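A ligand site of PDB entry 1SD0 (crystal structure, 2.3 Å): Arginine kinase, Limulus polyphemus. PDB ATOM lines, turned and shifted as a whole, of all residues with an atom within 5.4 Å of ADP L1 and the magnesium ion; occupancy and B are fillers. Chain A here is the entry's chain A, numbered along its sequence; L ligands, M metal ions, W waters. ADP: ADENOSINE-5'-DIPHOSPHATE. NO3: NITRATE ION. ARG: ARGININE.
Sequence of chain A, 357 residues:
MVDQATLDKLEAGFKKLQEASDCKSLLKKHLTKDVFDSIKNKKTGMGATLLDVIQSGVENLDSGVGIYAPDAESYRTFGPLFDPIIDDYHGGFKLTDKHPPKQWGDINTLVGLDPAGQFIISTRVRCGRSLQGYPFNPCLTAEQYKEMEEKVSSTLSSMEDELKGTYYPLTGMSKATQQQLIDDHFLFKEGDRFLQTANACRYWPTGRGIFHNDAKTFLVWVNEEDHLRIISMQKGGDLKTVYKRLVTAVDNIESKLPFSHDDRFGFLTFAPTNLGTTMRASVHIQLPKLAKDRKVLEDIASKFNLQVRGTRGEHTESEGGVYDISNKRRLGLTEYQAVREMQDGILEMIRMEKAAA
The guanidinium group (NE) of Arg 280 lies within salt-bridge range of an oxygen (O3B) of ADP L1. A ring nitrogen (ND1) of His 185 lies within hydrogen-bond range of an oxygen (O2') of ADP L1, 3.0 Å away. An oxygen (O2B) of ADP L1 is in salt-bridge range of the guanidinium group of Arg 124 (2.9 Å). The guanidinium group of Arg 126 is in salt-bridge range of an oxygen (O3B) of ADP L1 (2.7 Å). O2A of ADP L1 lies within hydrogen-bond range of N of Glu 314. The side-chain hydroxyl (OG) of Ser 282 sits at hydrogen-bond distance from a nitrogen (N7) of ADP L1 (2.6 Å). The backbone carbonyl oxygen (O) of Thr 311 lies within hydrogen-bond range of an oxygen (O2') of ADP L1, at 2.8 Å. O of Ser 282 sits at hydrogen-bond distance from N6 of ADP L1 (3.4 Å). The backbone carbonyl oxygen (O) of Ser 122 is in hydrogen-bond range of a nitrogen (N6) of ADP L1, at 3.4 Å. OE1 of Glu 314 is in salt-bridge range of NE of ARG L3, 2.8 Å away. A nitrogen (N1) of ADP L1 lies within hydrogen-bond range of the side-chain hydroxyl (OG) of Ser 122 (2.8 Å). OE2 of Glu 225 lies within salt-bridge range of NH2 of ARG L3 (2.6 Å). The guanidinium group of Arg 309 is in salt-bridge range of an oxygen (O2A) of ADP L1 (2.8 Å). An oxygen (O2B) of ADP L1 is in salt-bridge range of the guanidinium group of Arg 229.
The guanidinium group of Arg 229 is in salt-bridge range of the side-chain carboxylate of Glu 225 (3.7 Å). N of Arg 280 is in hydrogen-bond range of O of Arg 126. The guanidinium group (NE) of Arg 124 sits close to the side-chain sulfur (SD) of Met 233 (3.7 Å). NH2 of Arg 309 lies within salt-bridge range of OE1 of Glu 314. NH2 of Arg 280 lies within salt-bridge range of OD2 of Asp 324, at 3.0 Å. NE1 of Trp 221 is in hydrogen-bond range of O of Phe 186. The backbone carbonyl oxygen (O) of Ser 122 lies within hydrogen-bond range of the backbone NH (N) of His 284, at 2.9 Å. N of Arg 309 is in hydrogen-bond range of O of Asp 324 (2.7 Å).
N6 of ADP L1 sits close to N of Val 283 (3.4 Å). The backbone NH (N) of His 284 sits close to a nitrogen (N6) of ADP L1. The side-chain carboxylate (OD2) of Asp 324 lies close to a nitrogen (N7) of ADP L1, at 3.4 Å. Residues that only touch ADP L1: Trp 221, Met 233, Arg 312 and Gly 313. Hydrophobic or aromatic side chains within 4 Å of ADP L1: His 185, Trp 221, Met 233 and His 284. 17 residues have an atom within 4 Å of ADP L1: Ser 122, Arg 124, Arg 126, His 185, Trp 221, Arg 229, Met 233, Arg 280, Ser 282, Val 283, His 284, Arg 309, Thr 311, Arg 312, Gly 313, Glu 314 and Asp 324.
Residues that only touch the magnesium ion: Glu 224 (3.9 Å). Of the 25 residues printed, 1 comes within 4 Å of the magnesium ion.
The magnesium ion is bound by water W4 (1.9 Å), water W6 (2.0 Å), an oxygen (O1B) of ADP L1 (2.1 Å), an oxygen (O1) of NO3 L2 (2.1 Å), an oxygen (O1A) of ADP L1 (2.2 Å) and water W9 (2.3 Å). The magnesium ion has six donor atoms within binding distance.
Water W4 lies within hydrogen-bond range of OE2 of Glu 225 (2.8 Å) and OE1 of Glu 224 (2.9 Å). Water W10 lies within hydrogen-bond range of an oxygen (O3') of ADP L1 (2.6 Å), the backbone carbonyl oxygen (O) of Ile 182 (2.9 Å) and a ring nitrogen (ND1) of His 185 (3.1 Å). Water W2 lies within hydrogen-bond range of O2B of ADP L1 (2.6 Å) and NH1 of Arg 229 (2.9 Å). Water W3 lies within hydrogen-bond range of O of Leu 187 (2.7 Å) and O3' of ADP L1 (2.7 Å).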
ATOM      1  N   SER A 122       0.182  18.884   7.059  1.00  0.00           N
ATOM      2  CA  SER A 122       1.095  19.438   8.045  1.00  0.00           C
ATOM      3  C   SER A 122       2.102  18.398   8.545  1.00  0.00           C
ATOM      4  O   SER A 122       1.870  17.199   8.467  1.00  0.00           O
ATOM      5  CB  SER A 122       0.306  20.014   9.225  1.00  0.00           C
ATOM      6  OG  SER A 122      -0.539  19.019   9.789  1.00  0.00           O
ATOM      7  N   THR A 123       3.222  18.899   9.059  1.00  0.00           N
ATOM      8  CA  THR A 123       4.296  18.043   9.557  1.00  0.00           C
ATOM      9  C   THR A 123       4.594  18.320  11.027  1.00  0.00           C
ATOM     10  O   THR A 123       4.582  19.468  11.459  1.00  0.00           O
ATOM     11  CB  THR A 123       5.574  18.268   8.736  1.00  0.00           C
ATOM     12  OG1 THR A 123       5.282  18.037   7.355  1.00  0.00           O
ATOM     13  CG2 THR A 123       6.671  17.307   9.184  1.00  0.00           C
ATOM     14  N   ARG A 124       4.868  17.262  11.783  1.00  0.00           N
ATOM     15  CA  ARG A 124       5.133  17.390  13.216  1.00  0.00           C
ATOM     16  C   ARG A 124       6.100  16.345  13.735  1.00  0.00           C
ATOM     17  O   ARG A 124       6.084  15.197  13.305  1.00  0.00           O
ATOM     18  CB  ARG A 124       3.802  17.274  13.962  1.00  0.00           C
ATOM     19  CG  ARG A 124       3.831  17.249  15.486  1.00  0.00           C
ATOM     20  CD  ARG A 124       2.366  17.179  15.938  1.00  0.00           C
ATOM     21  NE  ARG A 124       2.083  17.122  17.375  1.00  0.00           N
ATOM     22  CZ  ARG A 124       2.195  16.037  18.138  1.00  0.00           C
ATOM     23  NH1 ARG A 124       2.611  14.889  17.613  1.00  0.00           N
ATOM     24  NH2 ARG A 124       1.816  16.078  19.401  1.00  0.00           N
ATOM     25  N   ARG A 126       7.886  15.071  17.583  1.00  0.00           N
ATOM     26  CA  ARG A 126       7.933  15.230  19.036  1.00  0.00           C
ATOM     27  C   ARG A 126       8.841  14.233  19.722  1.00  0.00           C
ATOM     28  O   ARG A 126       9.186  13.184  19.168  1.00  0.00           O
ATOM     29  CB  ARG A 126       6.522  15.137  19.647  1.00  0.00           C
ATOM     30  CG  ARG A 126       5.757  13.793  19.493  1.00  0.00           C
ATOM     31  CD  ARG A 126       6.280  12.647  20.380  1.00  0.00           C
ATOM     32  NE  ARG A 126       5.311  11.556  20.491  1.00  0.00           N
ATOM     33  CZ  ARG A 126       5.588  10.328  20.914  1.00  0.00           C
ATOM     34  NH1 ARG A 126       4.624   9.404  20.978  1.00  0.00           N
ATOM     35  NH2 ARG A 126       6.821   9.994  21.268  1.00  0.00           N
ATOM     36  N   ILE A 182      -7.130  21.709  21.253  1.00  0.00           N
ATOM     37  CA  ILE A 182      -7.200  20.281  21.006  1.00  0.00           C
ATOM     38  C   ILE A 182      -7.644  20.063  19.566  1.00  0.00           C
ATOM     39  O   ILE A 182      -7.067  19.235  18.846  1.00  0.00           O
ATOM     40  CB  ILE A 182      -8.205  19.598  21.951  1.00  0.00           C
ATOM     41  CG1 ILE A 182      -7.665  19.618  23.378  1.00  0.00           C
ATOM     42  CG2 ILE A 182      -8.490  18.170  21.473  1.00  0.00           C
ATOM     43  CD1 ILE A 182      -8.621  19.045  24.400  1.00  0.00           C
ATOM     44  N   HIS A 185      -5.070  20.526  16.974  1.00  0.00           N
ATOM     45  CA  HIS A 185      -3.984  19.550  17.062  1.00  0.00           C
ATOM     46  C   HIS A 185      -2.761  20.006  17.847  1.00  0.00           C
ATOM     47  O   HIS A 185      -1.665  19.443  17.698  1.00  0.00           O
ATOM     48  CB  HIS A 185      -3.571  19.132  15.650  1.00  0.00           C
ATOM     49  CG  HIS A 185      -4.735  18.784  14.781  1.00  0.00           C
ATOM     50  ND1 HIS A 185      -5.593  17.746  15.056  1.00  0.00           N
ATOM     51  CD2 HIS A 185      -5.211  19.379  13.659  1.00  0.00           C
ATOM     52  CE1 HIS A 185      -6.544  17.707  14.145  1.00  0.00           C
ATOM     53  NE2 HIS A 185      -6.330  18.689  13.282  1.00  0.00           N
ATOM     54  N   PHE A 186      -2.930  21.010  18.693  1.00  0.00           N
ATOM     55  CA  PHE A 186      -1.832  21.543  19.494  1.00  0.00           C
ATOM     56  C   PHE A 186      -1.783  20.974  20.904  1.00  0.00           C
ATOM     57  O   PHE A 186      -0.716  20.632  21.414  1.00  0.00           O
ATOM     58  CB  PHE A 186      -1.936  23.069  19.561  1.00  0.00           C
ATOM     59  CG  PHE A 186      -1.830  23.747  18.233  1.00  0.00           C
ATOM     60  CD1 PHE A 186      -2.737  24.741  17.870  1.00  0.00           C
ATOM     61  CD2 PHE A 186      -0.827  23.402  17.327  1.00  0.00           C
ATOM     62  CE1 PHE A 186      -2.652  25.379  16.634  1.00  0.00           C
ATOM     63  CE2 PHE A 186      -0.737  24.029  16.087  1.00  0.00           C
ATOM     64  CZ  PHE A 186      -1.649  25.024  15.736  1.00  0.00           C
ATOM     65  N   LEU A 187      -2.944  20.867  21.544  1.00  0.00           N
ATOM     66  CA  LEU A 187      -3.046  20.374  22.910  1.00  0.00           C
ATOM     67  C   LEU A 187      -3.495  18.919  23.021  1.00  0.00           C
ATOM     68  O   LEU A 187      -4.349  18.453  22.251  1.00  0.00           O
ATOM     69  CB  LEU A 187      -4.006  21.254  23.710  1.00  0.00           C
ATOM     70  CG  LEU A 187      -4.183  20.896  25.195  1.00  0.00           C
ATOM     71  CD1 LEU A 187      -2.887  21.160  25.941  1.00  0.00           C
ATOM     72  CD2 LEU A 187      -5.316  21.735  25.779  1.00  0.00           C
ATOM     73  N   TRP A 221       4.217  19.907  26.063  1.00  0.00           N
ATOM     74  CA  TRP A 221       3.109  19.356  26.846  1.00  0.00           C
ATOM     75  C   TRP A 221       3.671  19.070  28.233  1.00  0.00           C
ATOM     76  O   TRP A 221       4.722  18.436  28.362  1.00  0.00           O
ATOM     77  CB  TRP A 221       2.598  18.040  26.256  1.00  0.00           C
ATOM     78  CG  TRP A 221       1.734  18.170  25.030  1.00  0.00           C
ATOM     79  CD1 TRP A 221       1.364  19.328  24.407  1.00  0.00           C
ATOM     80  CD2 TRP A 221       1.151  17.095  24.284  1.00  0.00           C
ATOM     81  NE1 TRP A 221       0.581  19.037  23.306  1.00  0.00           N
ATOM     82  CE2 TRP A 221       0.437  17.681  23.211  1.00  0.00           C
ATOM     83  CE3 TRP A 221       1.150  15.699  24.416  1.00  0.00           C
ATOM     84  CZ2 TRP A 221      -0.269  16.917  22.273  1.00  0.00           C
ATOM     85  CZ3 TRP A 221       0.459  14.941  23.485  1.00  0.00           C
ATOM     86  CH2 TRP A 221      -0.240  15.550  22.419  1.00  0.00           C
ATOM     87  N   GLU A 224       1.298  15.059  30.768  1.00  0.00           N
ATOM     88  CA  GLU A 224       0.226  14.291  30.171  1.00  0.00           C
ATOM     89  C   GLU A 224       0.744  12.861  30.336  1.00  0.00           C
ATOM     90  O   GLU A 224       1.002  12.425  31.460  1.00  0.00           O
ATOM     91  CB  GLU A 224       0.054  14.624  28.682  1.00  0.00           C
ATOM     92  CG  GLU A 224      -1.202  13.997  28.072  1.00  0.00           C
ATOM     93  CD  GLU A 224      -0.907  13.144  26.861  1.00  0.00           C
ATOM     94  OE1 GLU A 224       0.247  12.679  26.722  1.00  0.00           O
ATOM     95  OE2 GLU A 224      -1.825  12.932  26.047  1.00  0.00           O
ATOM     96  N   GLU A 225       0.927  12.143  29.234  1.00  0.00           N
ATOM     97  CA  GLU A 225       1.442  10.787  29.333  1.00  0.00           C
ATOM     98  C   GLU A 225       2.852  10.788  29.926  1.00  0.00           C
ATOM     99  O   GLU A 225       3.207   9.891  30.695  1.00  0.00           O
ATOM    100  CB  GLU A 225       1.430  10.108  27.969  1.00  0.00           C
ATOM    101  CG  GLU A 225       2.038   8.716  27.989  1.00  0.00           C
ATOM    102  CD  GLU A 225       1.825   7.948  26.694  1.00  0.00           C
ATOM    103  OE1 GLU A 225       2.637   7.047  26.404  1.00  0.00           O
ATOM    104  OE2 GLU A 225       0.850   8.247  25.986  1.00  0.00           O
ATOM    105  N   ARG A 229       6.719  16.663  26.728  1.00  0.00           N
ATOM    106  CA  ARG A 229       6.617  16.269  25.339  1.00  0.00           C
ATOM    107  C   ARG A 229       7.027  17.544  24.606  1.00  0.00           C
ATOM    108  O   ARG A 229       6.313  18.540  24.659  1.00  0.00           O
ATOM    109  CB  ARG A 229       5.188  15.871  24.948  1.00  0.00           C
ATOM    110  CG  ARG A 229       4.775  14.472  25.376  1.00  0.00           C
ATOM    111  CD  ARG A 229       5.655  13.404  24.767  1.00  0.00           C
ATOM    112  NE  ARG A 229       5.220  12.074  25.159  1.00  0.00           N
ATOM    113  CZ  ARG A 229       4.142  11.463  24.659  1.00  0.00           C
ATOM    114  NH1 ARG A 229       3.412  12.074  23.743  1.00  0.00           N
ATOM    115  NH2 ARG A 229       3.789  10.259  25.089  1.00  0.00           N
ATOM    116  N   ILE A 231       7.326  19.412  21.363  1.00  0.00           N
ATOM    117  CA  ILE A 231       6.721  19.371  20.031  1.00  0.00           C
ATOM    118  C   ILE A 231       7.214  20.458  19.081  1.00  0.00           C
ATOM    119  O   ILE A 231       7.497  21.568  19.492  1.00  0.00           O
ATOM    120  CB  ILE A 231       5.192  19.580  20.124  1.00  0.00           C
ATOM    121  CG1 ILE A 231       4.611  18.773  21.286  1.00  0.00           C
ATOM    122  CG2 ILE A 231       4.527  19.193  18.799  1.00  0.00           C
ATOM    123  CD1 ILE A 231       4.782  17.297  21.141  1.00  0.00           C
ATOM    124  N   MET A 233       5.910  21.633  15.155  1.00  0.00           N
ATOM    125  CA  MET A 233       4.973  21.367  14.073  1.00  0.00           C
ATOM    126  C   MET A 233       4.600  22.628  13.289  1.00  0.00           C
ATOM    127  O   MET A 233       4.844  23.750  13.744  1.00  0.00           O
ATOM    128  CB  MET A 233       3.714  20.712  14.635  1.00  0.00           C
ATOM    129  CG  MET A 233       3.004  21.563  15.683  1.00  0.00           C
ATOM    130  SD  MET A 233       1.700  20.674  16.541  1.00  0.00           S
ATOM    131  CE  MET A 233       0.325  20.770  15.319  1.00  0.00           C
ATOM    132  N   ARG A 280       8.451  10.588  17.529  1.00  0.00           N
ATOM    133  CA  ARG A 280       7.343  10.223  16.657  1.00  0.00           C
ATOM    134  C   ARG A 280       7.270  11.344  15.628  1.00  0.00           C
ATOM    135  O   ARG A 280       6.772  12.433  15.919  1.00  0.00           O
ATOM    136  CB  ARG A 280       6.012  10.113  17.411  1.00  0.00           C
ATOM    137  CG  ARG A 280       4.888   9.482  16.559  1.00  0.00           C
ATOM    138  CD  ARG A 280       3.666   9.089  17.385  1.00  0.00           C
ATOM    139  NE  ARG A 280       2.608  10.106  17.389  1.00  0.00           N
ATOM    140  CZ  ARG A 280       1.857  10.404  16.342  1.00  0.00           C
ATOM    141  NH1 ARG A 280       2.038   9.772  15.189  1.00  0.00           N
ATOM    142  NH2 ARG A 280       0.911  11.340  16.432  1.00  0.00           N
ATOM    143  N   SER A 282       5.629  12.698  12.416  1.00  0.00           N
ATOM    144  CA  SER A 282       4.424  12.462  11.643  1.00  0.00           C
ATOM    145  C   SER A 282       4.035  13.565  10.666  1.00  0.00           C
ATOM    146  O   SER A 282       4.621  14.637  10.635  1.00  0.00           O
ATOM    147  CB  SER A 282       3.232  12.243  12.577  1.00  0.00           C
ATOM    148  OG  SER A 282       2.813  13.472  13.155  1.00  0.00           O
ATOM    149  N   VAL A 283       3.019  13.245   9.877  1.00  0.00           N
ATOM    150  CA  VAL A 283       2.465  14.153   8.892  1.00  0.00           C
ATOM    151  C   VAL A 283       0.968  13.864   8.836  1.00  0.00           C
ATOM    152  O   VAL A 283       0.534  12.746   9.099  1.00  0.00           O
ATOM    153  CB  VAL A 283       3.036  13.890   7.491  1.00  0.00           C
ATOM    154  CG1 VAL A 283       4.496  14.322   7.409  1.00  0.00           C
ATOM    155  CG2 VAL A 283       2.888  12.410   7.152  1.00  0.00           C
ATOM    156  N   HIS A 284       0.186  14.886   8.517  1.00  0.00           N
ATOM    157  CA  HIS A 284      -1.239  14.699   8.345  1.00  0.00           C
ATOM    158  C   HIS A 284      -1.289  14.683   6.826  1.00  0.00           C
ATOM    159  O   HIS A 284      -1.040  15.701   6.169  1.00  0.00           O
ATOM    160  CB  HIS A 284      -2.032  15.846   8.963  1.00  0.00           C
ATOM    161  CG  HIS A 284      -2.564  15.520  10.330  1.00  0.00           C
ATOM    162  ND1 HIS A 284      -3.375  16.380  11.046  1.00  0.00           N
ATOM    163  CD2 HIS A 284      -2.432  14.412  11.096  1.00  0.00           C
ATOM    164  CE1 HIS A 284      -3.714  15.806  12.180  1.00  0.00           C
ATOM    165  NE2 HIS A 284      -3.158  14.611  12.234  1.00  0.00           N
ATOM    166  N   ARG A 309      -2.673   6.636  12.142  1.00  0.00           N
ATOM    167  CA  ARG A 309      -3.564   7.073  13.219  1.00  0.00           C
ATOM    168  C   ARG A 309      -4.648   7.992  12.652  1.00  0.00           C
ATOM    169  O   ARG A 309      -4.523   8.482  11.534  1.00  0.00           O
ATOM    170  CB  ARG A 309      -2.762   7.826  14.306  1.00  0.00           C
ATOM    171  CG  ARG A 309      -1.822   6.952  15.124  1.00  0.00           C
ATOM    172  CD  ARG A 309      -0.938   7.766  16.060  1.00  0.00           C
ATOM    173  NE  ARG A 309       0.001   6.890  16.768  1.00  0.00           N
ATOM    174  CZ  ARG A 309       0.500   7.134  17.975  1.00  0.00           C
ATOM    175  NH1 ARG A 309       0.149   8.230  18.644  1.00  0.00           N
ATOM    176  NH2 ARG A 309       1.323   6.264  18.539  1.00  0.00           N
ATOM    177  N   GLY A 310      -5.696   8.220  13.436  1.00  0.00           N
ATOM    178  CA  GLY A 310      -6.780   9.083  12.996  1.00  0.00           C
ATOM    179  C   GLY A 310      -6.358  10.539  12.998  1.00  0.00           C
ATOM    180  O   GLY A 310      -5.266  10.860  13.446  1.00  0.00           O
ATOM    181  N   THR A 311      -7.225  11.422  12.514  1.00  0.00           N
ATOM    182  CA  THR A 311      -6.892  12.838  12.465  1.00  0.00           C
ATOM    183  C   THR A 311      -6.703  13.496  13.829  1.00  0.00           C
ATOM    184  O   THR A 311      -5.965  14.471  13.968  1.00  0.00           O
ATOM    185  CB  THR A 311      -7.938  13.644  11.667  1.00  0.00           C
ATOM    186  OG1 THR A 311      -8.272  12.937  10.461  1.00  0.00           O
ATOM    187  CG2 THR A 311      -7.381  15.008  11.279  1.00  0.00           C
ATOM    188  N   ARG A 312      -7.360  12.960  14.862  1.00  0.00           N
ATOM    189  CA  ARG A 312      -7.245  13.545  16.199  1.00  0.00           C
ATOM    190  C   ARG A 312      -6.263  12.780  17.083  1.00  0.00           C
ATOM    191  O   ARG A 312      -6.218  12.977  18.297  1.00  0.00           O
ATOM    192  CB  ARG A 312      -8.622  13.614  16.864  1.00  0.00           C
ATOM    193  CG  ARG A 312      -9.666  14.315  16.006  1.00  0.00           C
ATOM    194  CD  ARG A 312     -11.073  14.193  16.589  1.00  0.00           C
ATOM    195  NE  ARG A 312     -11.272  15.056  17.737  1.00  0.00           N
ATOM    196  CZ  ARG A 312     -11.303  16.384  17.669  1.00  0.00           C
ATOM    197  NH1 ARG A 312     -11.144  17.005  16.502  1.00  0.00           N
ATOM    198  NH2 ARG A 312     -11.472  17.102  18.771  1.00  0.00           N
ATOM    199  N   GLY A 313      -5.488  11.887  16.468  1.00  0.00           N
ATOM    200  CA  GLY A 313      -4.503  11.104  17.204  1.00  0.00           C
ATOM    201  C   GLY A 313      -4.825   9.624  17.213  1.00  0.00           C
ATOM    202  O   GLY A 313      -5.783   9.184  16.580  1.00  0.00           O
ATOM    203  N   GLU A 314      -4.025   8.849  17.945  1.00  0.00           N
ATOM    204  CA  GLU A 314      -4.227   7.403  18.043  1.00  0.00           C
ATOM    205  C   GLU A 314      -5.634   7.101  18.558  1.00  0.00           C
ATOM    206  O   GLU A 314      -6.267   7.940  19.188  1.00  0.00           O
ATOM    207  CB  GLU A 314      -3.183   6.788  18.986  1.00  0.00           C
ATOM    208  CG  GLU A 314      -3.254   7.318  20.415  1.00  0.00           C
ATOM    209  CD  GLU A 314      -2.262   6.635  21.325  1.00  0.00           C
ATOM    210  OE1 GLU A 314      -1.555   5.727  20.851  1.00  0.00           O
ATOM    211  OE2 GLU A 314      -2.181   7.016  22.515  1.00  0.00           O
ATOM    212  N   ASP A 324      -2.910  10.283   9.954  1.00  0.00           N
ATOM    213  CA  ASP A 324      -1.698  10.583  10.705  1.00  0.00           C
ATOM    214  C   ASP A 324      -0.760   9.402  10.433  1.00  0.00           C
ATOM    215  O   ASP A 324      -0.996   8.290  10.911  1.00  0.00           O
ATOM    216  CB  ASP A 324      -2.053  10.660  12.198  1.00  0.00           C
ATOM    217  CG  ASP A 324      -0.846  10.875  13.098  1.00  0.00           C
ATOM    218  OD1 ASP A 324       0.232  10.328  12.790  1.00  0.00           O
ATOM    219  OD2 ASP A 324      -0.978  11.574  14.124  1.00  0.00           O
HETATM  220  PB  ADP L   1       1.581  11.945  20.406  1.00  0.00           P
HETATM  221  O1B ADP L   1       1.114  11.607  21.789  1.00  0.00           O
HETATM  222  O2B ADP L   1       2.006  13.371  20.355  1.00  0.00           O
HETATM  223  O3B ADP L   1       2.676  11.072  19.900  1.00  0.00           O
HETATM  224  PA  ADP L   1      -1.223  11.448  19.528  1.00  0.00           P
HETATM  225  O1A ADP L   1      -1.527  11.340  20.979  1.00  0.00           O
HETATM  226  O2A ADP L   1      -1.690  10.353  18.626  1.00  0.00           O
HETATM  227  O3A ADP L   1       0.375  11.665  19.344  1.00  0.00           O
HETATM  228  O5' ADP L   1      -1.750  12.869  18.950  1.00  0.00           O
HETATM  229  C5' ADP L   1      -1.664  14.066  19.759  1.00  0.00           C
HETATM  230  C4' ADP L   1      -2.113  15.263  18.916  1.00  0.00           C
HETATM  231  O4' ADP L   1      -1.135  15.420  17.871  1.00  0.00           O
HETATM  232  C3' ADP L   1      -3.424  15.103  18.146  1.00  0.00           C
HETATM  233  O3' ADP L   1      -4.058  16.397  18.076  1.00  0.00           O
HETATM  234  C2' ADP L   1      -2.996  14.841  16.706  1.00  0.00           C
HETATM  235  O2' ADP L   1      -4.012  15.305  15.795  1.00  0.00           O
HETATM  236  C1' ADP L   1      -1.786  15.732  16.621  1.00  0.00           C
HETATM  237  N9  ADP L   1      -0.864  15.507  15.461  1.00  0.00           N
HETATM  238  C8  ADP L   1      -0.086  14.433  15.212  1.00  0.00           C
HETATM  239  N7  ADP L   1       0.645  14.615  14.095  1.00  0.00           N
HETATM  240  C5  ADP L   1       0.289  15.816  13.650  1.00  0.00           C
HETATM  241  C6  ADP L   1       0.647  16.330  12.408  1.00  0.00           C
HETATM  242  N6  ADP L   1       1.493  15.745  11.540  1.00  0.00           N
HETATM  243  N1  ADP L   1       0.015  17.489  12.090  1.00  0.00           N
HETATM  244  C2  ADP L   1      -0.855  18.056  12.923  1.00  0.00           C
HETATM  245  N3  ADP L   1      -1.183  17.541  14.101  1.00  0.00           N
HETATM  246  C4  ADP L   1      -0.631  16.390  14.483  1.00  0.00           C
HETATM  247  N   NO3 L   2       1.436   8.654  21.946  1.00  0.00           N
HETATM  248  O1  NO3 L   2       0.261   9.537  21.722  1.00  0.00           O
HETATM  249  O2  NO3 L   2       1.873   7.617  20.980  1.00  0.00           O
HETATM  250  O3  NO3 L   2       2.240   8.808  23.169  1.00  0.00           O
HETATM  251  N   ARG L   3      -2.082   1.997  25.917  1.00  0.00           N
HETATM  252  CA  ARG L   3      -2.553   2.219  24.519  1.00  0.00           C
HETATM  253  C   ARG L   3      -2.636   0.890  23.768  1.00  0.00           C
HETATM  254  O   ARG L   3      -1.872  -0.039  24.108  1.00  0.00           O
HETATM  255  CB  ARG L   3      -1.616   3.159  23.765  1.00  0.00           C
HETATM  256  CG  ARG L   3      -0.191   2.627  23.555  1.00  0.00           C
HETATM  257  CD  ARG L   3       0.551   3.409  22.472  1.00  0.00           C
HETATM  258  NE  ARG L   3       0.425   4.856  22.647  1.00  0.00           N
HETATM  259  CZ  ARG L   3       0.930   5.542  23.669  1.00  0.00           C
HETATM  260  NH1 ARG L   3       1.621   4.921  24.621  1.00  0.00           N
HETATM  261  NH2 ARG L   3       0.725   6.851  23.753  1.00  0.00           N
HETATM  262  OXT ARG L   3      -3.461   0.803  22.833  1.00  0.00           O
HETATM  263 MG    MG M   1      -0.507  11.037  22.936  1.00  0.00          MG
HETATM  264  O   HOH W   1      -4.178  11.380  21.889  1.00  0.00           O
HETATM  265  O   HOH W   2       3.615  14.479  22.073  1.00  0.00           O
HETATM  266  O   HOH W   3      -4.917  16.319  20.687  1.00  0.00           O
HETATM  267  O   HOH W   4       0.240  10.642  24.659  1.00  0.00           O
HETATM  268  O   HOH W   5      -3.161  12.950  14.587  1.00  0.00           O
HETATM  269  O   HOH W   6      -1.889   9.682  23.284  1.00  0.00           O
HETATM  270  O   HOH W   7      -3.959  13.957  22.332  1.00  0.00           O
HETATM  271  O   HOH W   8      -2.371  20.612  11.082  1.00  0.00           O
HETATM  272  O   HOH W   9      -1.790  12.847  23.422  1.00  0.00           O
HETATM  273  O   HOH W  10      -6.581  16.642  17.739  1.00  0.00           O
